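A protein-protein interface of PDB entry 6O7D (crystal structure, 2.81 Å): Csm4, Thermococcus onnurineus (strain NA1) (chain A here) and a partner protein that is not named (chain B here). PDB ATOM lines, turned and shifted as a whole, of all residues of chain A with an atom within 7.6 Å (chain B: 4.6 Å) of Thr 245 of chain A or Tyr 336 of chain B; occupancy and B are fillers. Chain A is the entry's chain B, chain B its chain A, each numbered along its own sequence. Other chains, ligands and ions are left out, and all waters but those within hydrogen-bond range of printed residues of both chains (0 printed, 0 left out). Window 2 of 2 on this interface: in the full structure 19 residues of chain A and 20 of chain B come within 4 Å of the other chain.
The guanidinium group of Arg 231 of chain A lies within salt-bridge range of the side-chain carboxylate of Glu 340 of chain B.
O of Leu 391 of chain B is in hydrogen-bond range of OG1 of Thr 245 of chain A (3.3 Å).
Leu 229 of chain A touches Ser 341 of chain B.
Leu 229 of chain A touches Phe 385 of chain B.
CG2 of Thr 245 of chain A touches OH of Tyr 336 of chain B, 3.7 Å away.
Thr 245 of chain A touches two residues of chain B.
Tyr 336 of chain B touches just one residue of chain A: Thr 245.
Of the printed residues of chain A, Glu 340 of chain B touches Arg 231.
Of the printed residues of chain B, Arg 231 of chain A touches Glu 340 (3.2 Å).
Of the printed residues of chain B, Leu 229 of chain A touches Ser 341 and Phe 385.
Printed residues of chain A within 4 Å of Phe 385 of chain B: Leu 229 (3.7 Å).
Met 244 of chain A touches none of the printed residues of chain B.
The nearest printed residue of chain B that does not touch Thr 245 of chain A is Ser 341 of chain B (6.4 Å).
The nearest residue of chain A that does not touch Tyr 336 of chain B is Leu 229 of chain A (5.1 Å).
Of the 13 printed residues of chain B, 5 touch a printed residue of chain A.
Printed residues of chain B that touch a printed residue of chain A: Tyr 336, Glu 340, Ser 341, Phe 385 and Leu 391.
Along chain B the printed residues that touch a printed residue of chain A span positions 336 to 391.
Among the printed residues, 5 pairs touch across the chains.
Among the printed residues, Asp or Glu carboxylates within 4 Å of a Lys or Arg side-chain nitrogen of the other chain: Arg 231 of chain A with Glu 340 of chain B (3.2 Å).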
ATOM      1  N   ALA A 218       8.569 -34.715  19.402  1.00  0.00           N
ATOM      2  CA  ALA A 218       9.831 -34.594  20.173  1.00  0.00           C
ATOM      3  C   ALA A 218      10.564 -33.289  19.840  1.00  0.00           C
ATOM      4  O   ALA A 218      10.399 -32.775  18.716  1.00  0.00           O
ATOM      5  CB  ALA A 218      10.708 -35.788  19.890  1.00  0.00           C
ATOM      6  N   LEU A 219      11.338 -32.785  20.808  1.00  0.00           N
ATOM      7  CA  LEU A 219      12.392 -31.751  20.623  1.00  0.00           C
ATOM      8  C   LEU A 219      13.717 -32.477  20.420  1.00  0.00           C
ATOM      9  O   LEU A 219      14.342 -32.899  21.392  1.00  0.00           O
ATOM     10  CB  LEU A 219      12.465 -30.851  21.861  1.00  0.00           C
ATOM     11  CG  LEU A 219      11.155 -30.205  22.306  1.00  0.00           C
ATOM     12  CD1 LEU A 219      11.310 -29.587  23.687  1.00  0.00           C
ATOM     13  CD2 LEU A 219      10.689 -29.163  21.302  1.00  0.00           C
ATOM     14  N   PRO A 220      14.187 -32.667  19.167  1.00  0.00           N
ATOM     15  CA  PRO A 220      15.360 -33.506  18.919  1.00  0.00           C
ATOM     16  C   PRO A 220      16.648 -32.862  19.451  1.00  0.00           C
ATOM     17  O   PRO A 220      16.768 -31.651  19.387  1.00  0.00           O
ATOM     18  CB  PRO A 220      15.378 -33.631  17.391  1.00  0.00           C
ATOM     19  CG  PRO A 220      14.752 -32.338  16.927  1.00  0.00           C
ATOM     20  CD  PRO A 220      13.653 -32.067  17.934  1.00  0.00           C
ATOM     21  N   LEU A 229       8.391 -31.011  10.401  1.00  0.00           N
ATOM     22  CA  LEU A 229       8.365 -29.914  11.404  1.00  0.00           C
ATOM     23  C   LEU A 229       6.915 -29.643  11.809  1.00  0.00           C
ATOM     24  O   LEU A 229       6.006 -29.951  11.014  1.00  0.00           O
ATOM     25  CB  LEU A 229       9.011 -28.655  10.817  1.00  0.00           C
ATOM     26  CG  LEU A 229      10.520 -28.724  10.591  1.00  0.00           C
ATOM     27  CD1 LEU A 229      11.022 -27.437   9.957  1.00  0.00           C
ATOM     28  CD2 LEU A 229      11.262 -29.002  11.892  1.00  0.00           C
ATOM     29  N   LEU A 230       6.724 -29.073  12.999  1.00  0.00           N
ATOM     30  CA  LEU A 230       5.397 -28.867  13.634  1.00  0.00           C
ATOM     31  C   LEU A 230       5.503 -27.704  14.627  1.00  0.00           C
ATOM     32  O   LEU A 230       6.075 -27.904  15.717  1.00  0.00           O
ATOM     33  CB  LEU A 230       4.988 -30.182  14.305  1.00  0.00           C
ATOM     34  CG  LEU A 230       3.761 -30.137  15.212  1.00  0.00           C
ATOM     35  CD1 LEU A 230       2.550 -29.578  14.480  1.00  0.00           C
ATOM     36  CD2 LEU A 230       3.461 -31.523  15.761  1.00  0.00           C
ATOM     37  N   ARG A 231       4.979 -26.536  14.243  1.00  0.00           N
ATOM     38  CA  ARG A 231       5.186 -25.232  14.932  1.00  0.00           C
ATOM     39  C   ARG A 231       4.105 -25.036  16.003  1.00  0.00           C
ATOM     40  O   ARG A 231       2.926 -25.320  15.712  1.00  0.00           O
ATOM     41  CB  ARG A 231       5.159 -24.105  13.894  1.00  0.00           C
ATOM     42  CG  ARG A 231       5.714 -22.775  14.384  1.00  0.00           C
ATOM     43  CD  ARG A 231       7.173 -22.562  14.025  1.00  0.00           C
ATOM     44  NE  ARG A 231       7.601 -21.210  14.369  1.00  0.00           N
ATOM     45  CZ  ARG A 231       8.371 -20.875  15.406  1.00  0.00           C
ATOM     46  NH1 ARG A 231       8.842 -21.794  16.233  1.00  0.00           N
ATOM     47  NH2 ARG A 231       8.677 -19.604  15.604  1.00  0.00           N
ATOM     48  N   LYS A 232       4.504 -24.571  17.194  1.00  0.00           N
ATOM     49  CA  LYS A 232       3.596 -24.195  18.315  1.00  0.00           C
ATOM     50  C   LYS A 232       4.107 -22.906  18.969  1.00  0.00           C
ATOM     51  O   LYS A 232       3.249 -22.079  19.339  1.00  0.00           O
ATOM     52  CB  LYS A 232       3.500 -25.330  19.341  1.00  0.00           C
ATOM     53  CG  LYS A 232       2.604 -26.490  18.928  1.00  0.00           C
ATOM     54  CD  LYS A 232       2.412 -27.533  20.008  1.00  0.00           C
ATOM     55  CE  LYS A 232       1.514 -28.669  19.563  1.00  0.00           C
ATOM     56  NZ  LYS A 232       0.912 -29.380  20.716  1.00  0.00           N
ATOM     57  N   ARG A 243       6.965 -20.244  21.507  1.00  0.00           N
ATOM     58  CA  ARG A 243       6.864 -21.033  20.248  1.00  0.00           C
ATOM     59  C   ARG A 243       7.998 -22.065  20.195  1.00  0.00           C
ATOM     60  O   ARG A 243       9.174 -21.654  20.272  1.00  0.00           O
ATOM     61  CB  ARG A 243       6.901 -20.114  19.021  1.00  0.00           C
ATOM     62  CG  ARG A 243       5.644 -19.276  18.837  1.00  0.00           C
ATOM     63  CD  ARG A 243       5.500 -18.735  17.425  1.00  0.00           C
ATOM     64  NE  ARG A 243       4.296 -17.926  17.267  1.00  0.00           N
ATOM     65  CZ  ARG A 243       3.095 -18.383  16.904  1.00  0.00           C
ATOM     66  NH1 ARG A 243       2.904 -19.667  16.648  1.00  0.00           N
ATOM     67  NH2 ARG A 243       2.080 -17.540  16.798  1.00  0.00           N
ATOM     68  N   MET A 244       7.644 -23.350  20.072  1.00  0.00           N
ATOM     69  CA  MET A 244       8.587 -24.498  19.978  1.00  0.00           C
ATOM     70  C   MET A 244       8.536 -25.085  18.562  1.00  0.00           C
ATOM     71  O   MET A 244       7.431 -25.136  17.985  1.00  0.00           O
ATOM     72  CB  MET A 244       8.214 -25.602  20.974  1.00  0.00           C
ATOM     73  CG  MET A 244       8.142 -25.142  22.420  1.00  0.00           C
ATOM     74  SD  MET A 244       9.633 -24.278  22.983  1.00  0.00           S
ATOM     75  CE  MET A 244      10.918 -25.368  22.371  1.00  0.00           C
ATOM     76  N   THR A 245       9.688 -25.520  18.039  1.00  0.00           N
ATOM     77  CA  THR A 245       9.809 -26.316  16.787  1.00  0.00           C
ATOM     78  C   THR A 245       9.883 -27.801  17.161  1.00  0.00           C
ATOM     79  O   THR A 245      10.914 -28.218  17.724  1.00  0.00           O
ATOM     80  CB  THR A 245      11.011 -25.863  15.946  1.00  0.00           C
ATOM     81  OG1 THR A 245      12.170 -25.844  16.779  1.00  0.00           O
ATOM     82  CG2 THR A 245      10.812 -24.497  15.327  1.00  0.00           C
ATOM     83  N   PHE A 246       8.818 -28.556  16.871  1.00  0.00           N
ATOM     84  CA  PHE A 246       8.669 -29.996  17.211  1.00  0.00           C
ATOM     85  C   PHE A 246       8.853 -30.862  15.959  1.00  0.00           C
ATOM     86  O   PHE A 246       8.411 -30.463  14.864  1.00  0.00           O
ATOM     87  CB  PHE A 246       7.296 -30.277  17.831  1.00  0.00           C
ATOM     88  CG  PHE A 246       7.224 -30.128  19.330  1.00  0.00           C
ATOM     89  CD1 PHE A 246       7.598 -31.170  20.165  1.00  0.00           C
ATOM     90  CD2 PHE A 246       6.763 -28.953  19.906  1.00  0.00           C
ATOM     91  CE1 PHE A 246       7.524 -31.035  21.543  1.00  0.00           C
ATOM     92  CE2 PHE A 246       6.690 -28.821  21.284  1.00  0.00           C
ATOM     93  CZ  PHE A 246       7.071 -29.862  22.100  1.00  0.00           C
ATOM     94  N   ILE A 247       9.503 -32.013  16.139  1.00  0.00           N
ATOM     95  CA  ILE A 247       9.477 -33.183  15.211  1.00  0.00           C
ATOM     96  C   ILE A 247       8.107 -33.858  15.360  1.00  0.00           C
ATOM     97  O   ILE A 247       7.672 -34.036  16.511  1.00  0.00           O
ATOM     98  CB  ILE A 247      10.646 -34.141  15.535  1.00  0.00           C
ATOM     99  CG1 ILE A 247      11.918 -33.760  14.776  1.00  0.00           C
ATOM    100  CG2 ILE A 247      10.271 -35.593  15.286  1.00  0.00           C
ATOM    101  CD1 ILE A 247      13.079 -34.680  15.061  1.00  0.00           C
ATOM    102  N   ALA A 248       7.456 -34.219  14.251  1.00  0.00           N
ATOM    103  CA  ALA A 248       6.110 -34.843  14.234  1.00  0.00           C
ATOM    104  C   ALA A 248       6.215 -36.332  14.586  1.00  0.00           C
ATOM    105  O   ALA A 248       7.333 -36.883  14.518  1.00  0.00           O
ATOM    106  CB  ALA A 248       5.460 -34.651  12.886  1.00  0.00           C
ATOM    107  N   GLU A 261      12.216 -29.380  28.491  1.00  0.00           N
ATOM    108  CA  GLU A 261      12.608 -27.952  28.637  1.00  0.00           C
ATOM    109  C   GLU A 261      11.744 -27.298  29.721  1.00  0.00           C
ATOM    110  O   GLU A 261      10.508 -27.256  29.551  1.00  0.00           O
ATOM    111  CB  GLU A 261      12.479 -27.218  27.301  1.00  0.00           C
ATOM    112  CG  GLU A 261      13.617 -27.509  26.337  1.00  0.00           C
ATOM    113  CD  GLU A 261      13.541 -26.761  25.016  1.00  0.00           C
ATOM    114  OE1 GLU A 261      12.632 -25.921  24.866  1.00  0.00           O
ATOM    115  OE2 GLU A 261      14.392 -27.020  24.141  1.00  0.00           O
ATOM    116  N   VAL B 332      17.382 -21.149   1.575  1.00  0.00           N
ATOM    117  CA  VAL B 332      16.599 -21.825   2.656  1.00  0.00           C
ATOM    118  C   VAL B 332      16.653 -20.963   3.925  1.00  0.00           C
ATOM    119  O   VAL B 332      15.585 -20.734   4.525  1.00  0.00           O
ATOM    120  CB  VAL B 332      17.113 -23.255   2.919  1.00  0.00           C
ATOM    121  CG1 VAL B 332      16.625 -23.806   4.252  1.00  0.00           C
ATOM    122  CG2 VAL B 332      16.737 -24.200   1.789  1.00  0.00           C
ATOM    123  N   GLU B 333      17.851 -20.512   4.313  1.00  0.00           N
ATOM    124  CA  GLU B 333      18.088 -19.676   5.522  1.00  0.00           C
ATOM    125  C   GLU B 333      17.240 -18.401   5.445  1.00  0.00           C
ATOM    126  O   GLU B 333      16.695 -18.002   6.494  1.00  0.00           O
ATOM    127  CB  GLU B 333      19.574 -19.338   5.672  1.00  0.00           C
ATOM    128  CG  GLU B 333      20.375 -20.439   6.342  1.00  0.00           C
ATOM    129  CD  GLU B 333      21.877 -20.354   6.129  1.00  0.00           C
ATOM    130  OE1 GLU B 333      22.396 -19.225   6.017  1.00  0.00           O
ATOM    131  OE2 GLU B 333      22.526 -21.419   6.072  1.00  0.00           O
ATOM    132  N   TRP B 334      17.134 -17.791   4.258  1.00  0.00           N
ATOM    133  CA  TRP B 334      16.300 -16.580   4.025  1.00  0.00           C
ATOM    134  C   TRP B 334      14.818 -16.937   4.189  1.00  0.00           C
ATOM    135  O   TRP B 334      14.113 -16.179   4.880  1.00  0.00           O
ATOM    136  CB  TRP B 334      16.569 -15.946   2.656  1.00  0.00           C
ATOM    137  CG  TRP B 334      15.770 -14.697   2.435  1.00  0.00           C
ATOM    138  CD1 TRP B 334      16.081 -13.439   2.859  1.00  0.00           C
ATOM    139  CD2 TRP B 334      14.503 -14.591   1.763  1.00  0.00           C
ATOM    140  NE1 TRP B 334      15.103 -12.555   2.487  1.00  0.00           N
ATOM    141  CE2 TRP B 334      14.122 -13.231   1.813  1.00  0.00           C
ATOM    142  CE3 TRP B 334      13.658 -15.503   1.118  1.00  0.00           C
ATOM    143  CZ2 TRP B 334      12.937 -12.770   1.242  1.00  0.00           C
ATOM    144  CZ3 TRP B 334      12.485 -15.045   0.557  1.00  0.00           C
ATOM    145  CH2 TRP B 334      12.132 -13.696   0.618  1.00  0.00           C
ATOM    146  N   LEU B 335      14.369 -18.039   3.574  1.00  0.00           N
ATOM    147  CA  LEU B 335      12.961 -18.520   3.640  1.00  0.00           C
ATOM    148  C   LEU B 335      12.557 -18.717   5.106  1.00  0.00           C
ATOM    149  O   LEU B 335      11.432 -18.313   5.461  1.00  0.00           O
ATOM    150  CB  LEU B 335      12.805 -19.834   2.864  1.00  0.00           C
ATOM    151  CG  LEU B 335      12.945 -19.759   1.342  1.00  0.00           C
ATOM    152  CD1 LEU B 335      12.761 -21.136   0.724  1.00  0.00           C
ATOM    153  CD2 LEU B 335      11.956 -18.776   0.732  1.00  0.00           C
ATOM    154  N   TYR B 336      13.439 -19.314   5.919  1.00  0.00           N
ATOM    155  CA  TYR B 336      13.187 -19.638   7.349  1.00  0.00           C
ATOM    156  C   TYR B 336      13.032 -18.344   8.157  1.00  0.00           C
ATOM    157  O   TYR B 336      12.044 -18.224   8.905  1.00  0.00           O
ATOM    158  CB  TYR B 336      14.302 -20.504   7.941  1.00  0.00           C
ATOM    159  CG  TYR B 336      13.977 -21.046   9.310  1.00  0.00           C
ATOM    160  CD1 TYR B 336      14.368 -20.376  10.459  1.00  0.00           C
ATOM    161  CD2 TYR B 336      13.245 -22.214   9.460  1.00  0.00           C
ATOM    162  CE1 TYR B 336      14.058 -20.861  11.720  1.00  0.00           C
ATOM    163  CE2 TYR B 336      12.927 -22.713  10.713  1.00  0.00           C
ATOM    164  CZ  TYR B 336      13.336 -22.035  11.848  1.00  0.00           C
ATOM    165  OH  TYR B 336      13.026 -22.523  13.084  1.00  0.00           O
ATOM    166  N   ARG B 337      13.982 -17.415   8.007  1.00  0.00           N
ATOM    167  CA  ARG B 337      13.992 -16.097   8.701  1.00  0.00           C
ATOM    168  C   ARG B 337      12.737 -15.298   8.328  1.00  0.00           C
ATOM    169  O   ARG B 337      12.241 -14.550   9.194  1.00  0.00           O
ATOM    170  CB  ARG B 337      15.255 -15.308   8.340  1.00  0.00           C
ATOM    171  CG  ARG B 337      16.518 -15.852   8.991  1.00  0.00           C
ATOM    172  CD  ARG B 337      17.806 -15.368   8.349  1.00  0.00           C
ATOM    173  NE  ARG B 337      18.924 -16.231   8.713  1.00  0.00           N
ATOM    174  CZ  ARG B 337      20.213 -15.933   8.560  1.00  0.00           C
ATOM    175  NH1 ARG B 337      20.584 -14.771   8.046  1.00  0.00           N
ATOM    176  NH2 ARG B 337      21.133 -16.807   8.932  1.00  0.00           N
ATOM    177  N   GLU B 338      12.243 -15.463   7.096  1.00  0.00           N
ATOM    178  CA  GLU B 338      11.217 -14.580   6.481  1.00  0.00           C
ATOM    179  C   GLU B 338       9.802 -15.126   6.728  1.00  0.00           C
ATOM    180  O   GLU B 338       8.886 -14.290   6.855  1.00  0.00           O
ATOM    181  CB  GLU B 338      11.508 -14.411   4.987  1.00  0.00           C
ATOM    182  CG  GLU B 338      10.848 -13.191   4.367  1.00  0.00           C
ATOM    183  CD  GLU B 338      11.188 -11.865   5.030  1.00  0.00           C
ATOM    184  OE1 GLU B 338      10.286 -11.008   5.129  1.00  0.00           O
ATOM    185  OE2 GLU B 338      12.353 -11.693   5.444  1.00  0.00           O
ATOM    186  N   PHE B 339       9.616 -16.454   6.785  1.00  0.00           N
ATOM    187  CA  PHE B 339       8.273 -17.100   6.840  1.00  0.00           C
ATOM    188  C   PHE B 339       8.218 -18.324   7.769  1.00  0.00           C
ATOM    189  O   PHE B 339       7.151 -18.971   7.782  1.00  0.00           O
ATOM    190  CB  PHE B 339       7.841 -17.530   5.434  1.00  0.00           C
ATOM    191  CG  PHE B 339       7.953 -16.457   4.380  1.00  0.00           C
ATOM    192  CD1 PHE B 339       7.099 -15.366   4.386  1.00  0.00           C
ATOM    193  CD2 PHE B 339       8.912 -16.539   3.382  1.00  0.00           C
ATOM    194  CE1 PHE B 339       7.203 -14.378   3.418  1.00  0.00           C
ATOM    195  CE2 PHE B 339       9.015 -15.551   2.415  1.00  0.00           C
ATOM    196  CZ  PHE B 339       8.160 -14.475   2.433  1.00  0.00           C
ATOM    197  N   GLU B 340       9.282 -18.635   8.522  1.00  0.00           N
ATOM    198  CA  GLU B 340       9.377 -19.843   9.394  1.00  0.00           C
ATOM    199  C   GLU B 340       9.343 -21.097   8.505  1.00  0.00           C
ATOM    200  O   GLU B 340       9.872 -21.022   7.377  1.00  0.00           O
ATOM    201  CB  GLU B 340       8.266 -19.841  10.450  1.00  0.00           C
ATOM    202  CG  GLU B 340       8.154 -18.540  11.227  1.00  0.00           C
ATOM    203  CD  GLU B 340       6.784 -18.274  11.829  1.00  0.00           C
ATOM    204  OE1 GLU B 340       6.142 -19.241  12.290  1.00  0.00           O
ATOM    205  OE2 GLU B 340       6.360 -17.100  11.833  1.00  0.00           O
ATOM    206  N   SER B 341       8.737 -22.196   8.975  1.00  0.00           N
ATOM    207  CA  SER B 341       8.702 -23.509   8.274  1.00  0.00           C
ATOM    208  C   SER B 341       7.486 -23.604   7.338  1.00  0.00           C
ATOM    209  O   SER B 341       7.138 -24.738   6.950  1.00  0.00           O
ATOM    210  CB  SER B 341       8.726 -24.656   9.262  1.00  0.00           C
ATOM    211  OG  SER B 341       7.412 -25.079   9.597  1.00  0.00           O
ATOM    212  N   PHE B 385      14.349 -27.978   5.990  1.00  0.00           N
ATOM    213  CA  PHE B 385      15.205 -27.005   6.724  1.00  0.00           C
ATOM    214  C   PHE B 385      16.350 -27.744   7.431  1.00  0.00           C
ATOM    215  O   PHE B 385      16.884 -27.211   8.424  1.00  0.00           O
ATOM    216  CB  PHE B 385      14.363 -26.157   7.682  1.00  0.00           C
ATOM    217  CG  PHE B 385      13.333 -25.299   6.994  1.00  0.00           C
ATOM    218  CD1 PHE B 385      13.688 -24.079   6.437  1.00  0.00           C
ATOM    219  CD2 PHE B 385      12.015 -25.712   6.890  1.00  0.00           C
ATOM    220  CE1 PHE B 385      12.744 -23.288   5.801  1.00  0.00           C
ATOM    221  CE2 PHE B 385      11.073 -24.922   6.250  1.00  0.00           C
ATOM    222  CZ  PHE B 385      11.438 -23.711   5.708  1.00  0.00           C
ATOM    223  N   ILE B 388      19.835 -26.050   7.833  1.00  0.00           N
ATOM    224  CA  ILE B 388      20.023 -25.182   9.036  1.00  0.00           C
ATOM    225  C   ILE B 388      20.364 -26.093  10.221  1.00  0.00           C
ATOM    226  O   ILE B 388      19.568 -27.015  10.487  1.00  0.00           O
ATOM    227  CB  ILE B 388      18.749 -24.351   9.309  1.00  0.00           C
ATOM    228  CG1 ILE B 388      18.497 -23.310   8.212  1.00  0.00           C
ATOM    229  CG2 ILE B 388      18.795 -23.710  10.690  1.00  0.00           C
ATOM    230  CD1 ILE B 388      17.126 -22.674   8.270  1.00  0.00           C
ATOM    231  N   LEU B 391      18.272 -25.171  13.877  1.00  0.00           N
ATOM    232  CA  LEU B 391      16.817 -25.452  13.738  1.00  0.00           C
ATOM    233  C   LEU B 391      16.254 -25.972  15.067  1.00  0.00           C
ATOM    234  O   LEU B 391      15.110 -25.605  15.403  1.00  0.00           O
ATOM    235  CB  LEU B 391      16.612 -26.469  12.609  1.00  0.00           C
ATOM    236  CG  LEU B 391      15.179 -26.960  12.392  1.00  0.00           C
ATOM    237  CD1 LEU B 391      14.222 -25.798  12.164  1.00  0.00           C
ATOM    238  CD2 LEU B 391      15.118 -27.934  11.226  1.00  0.00           C
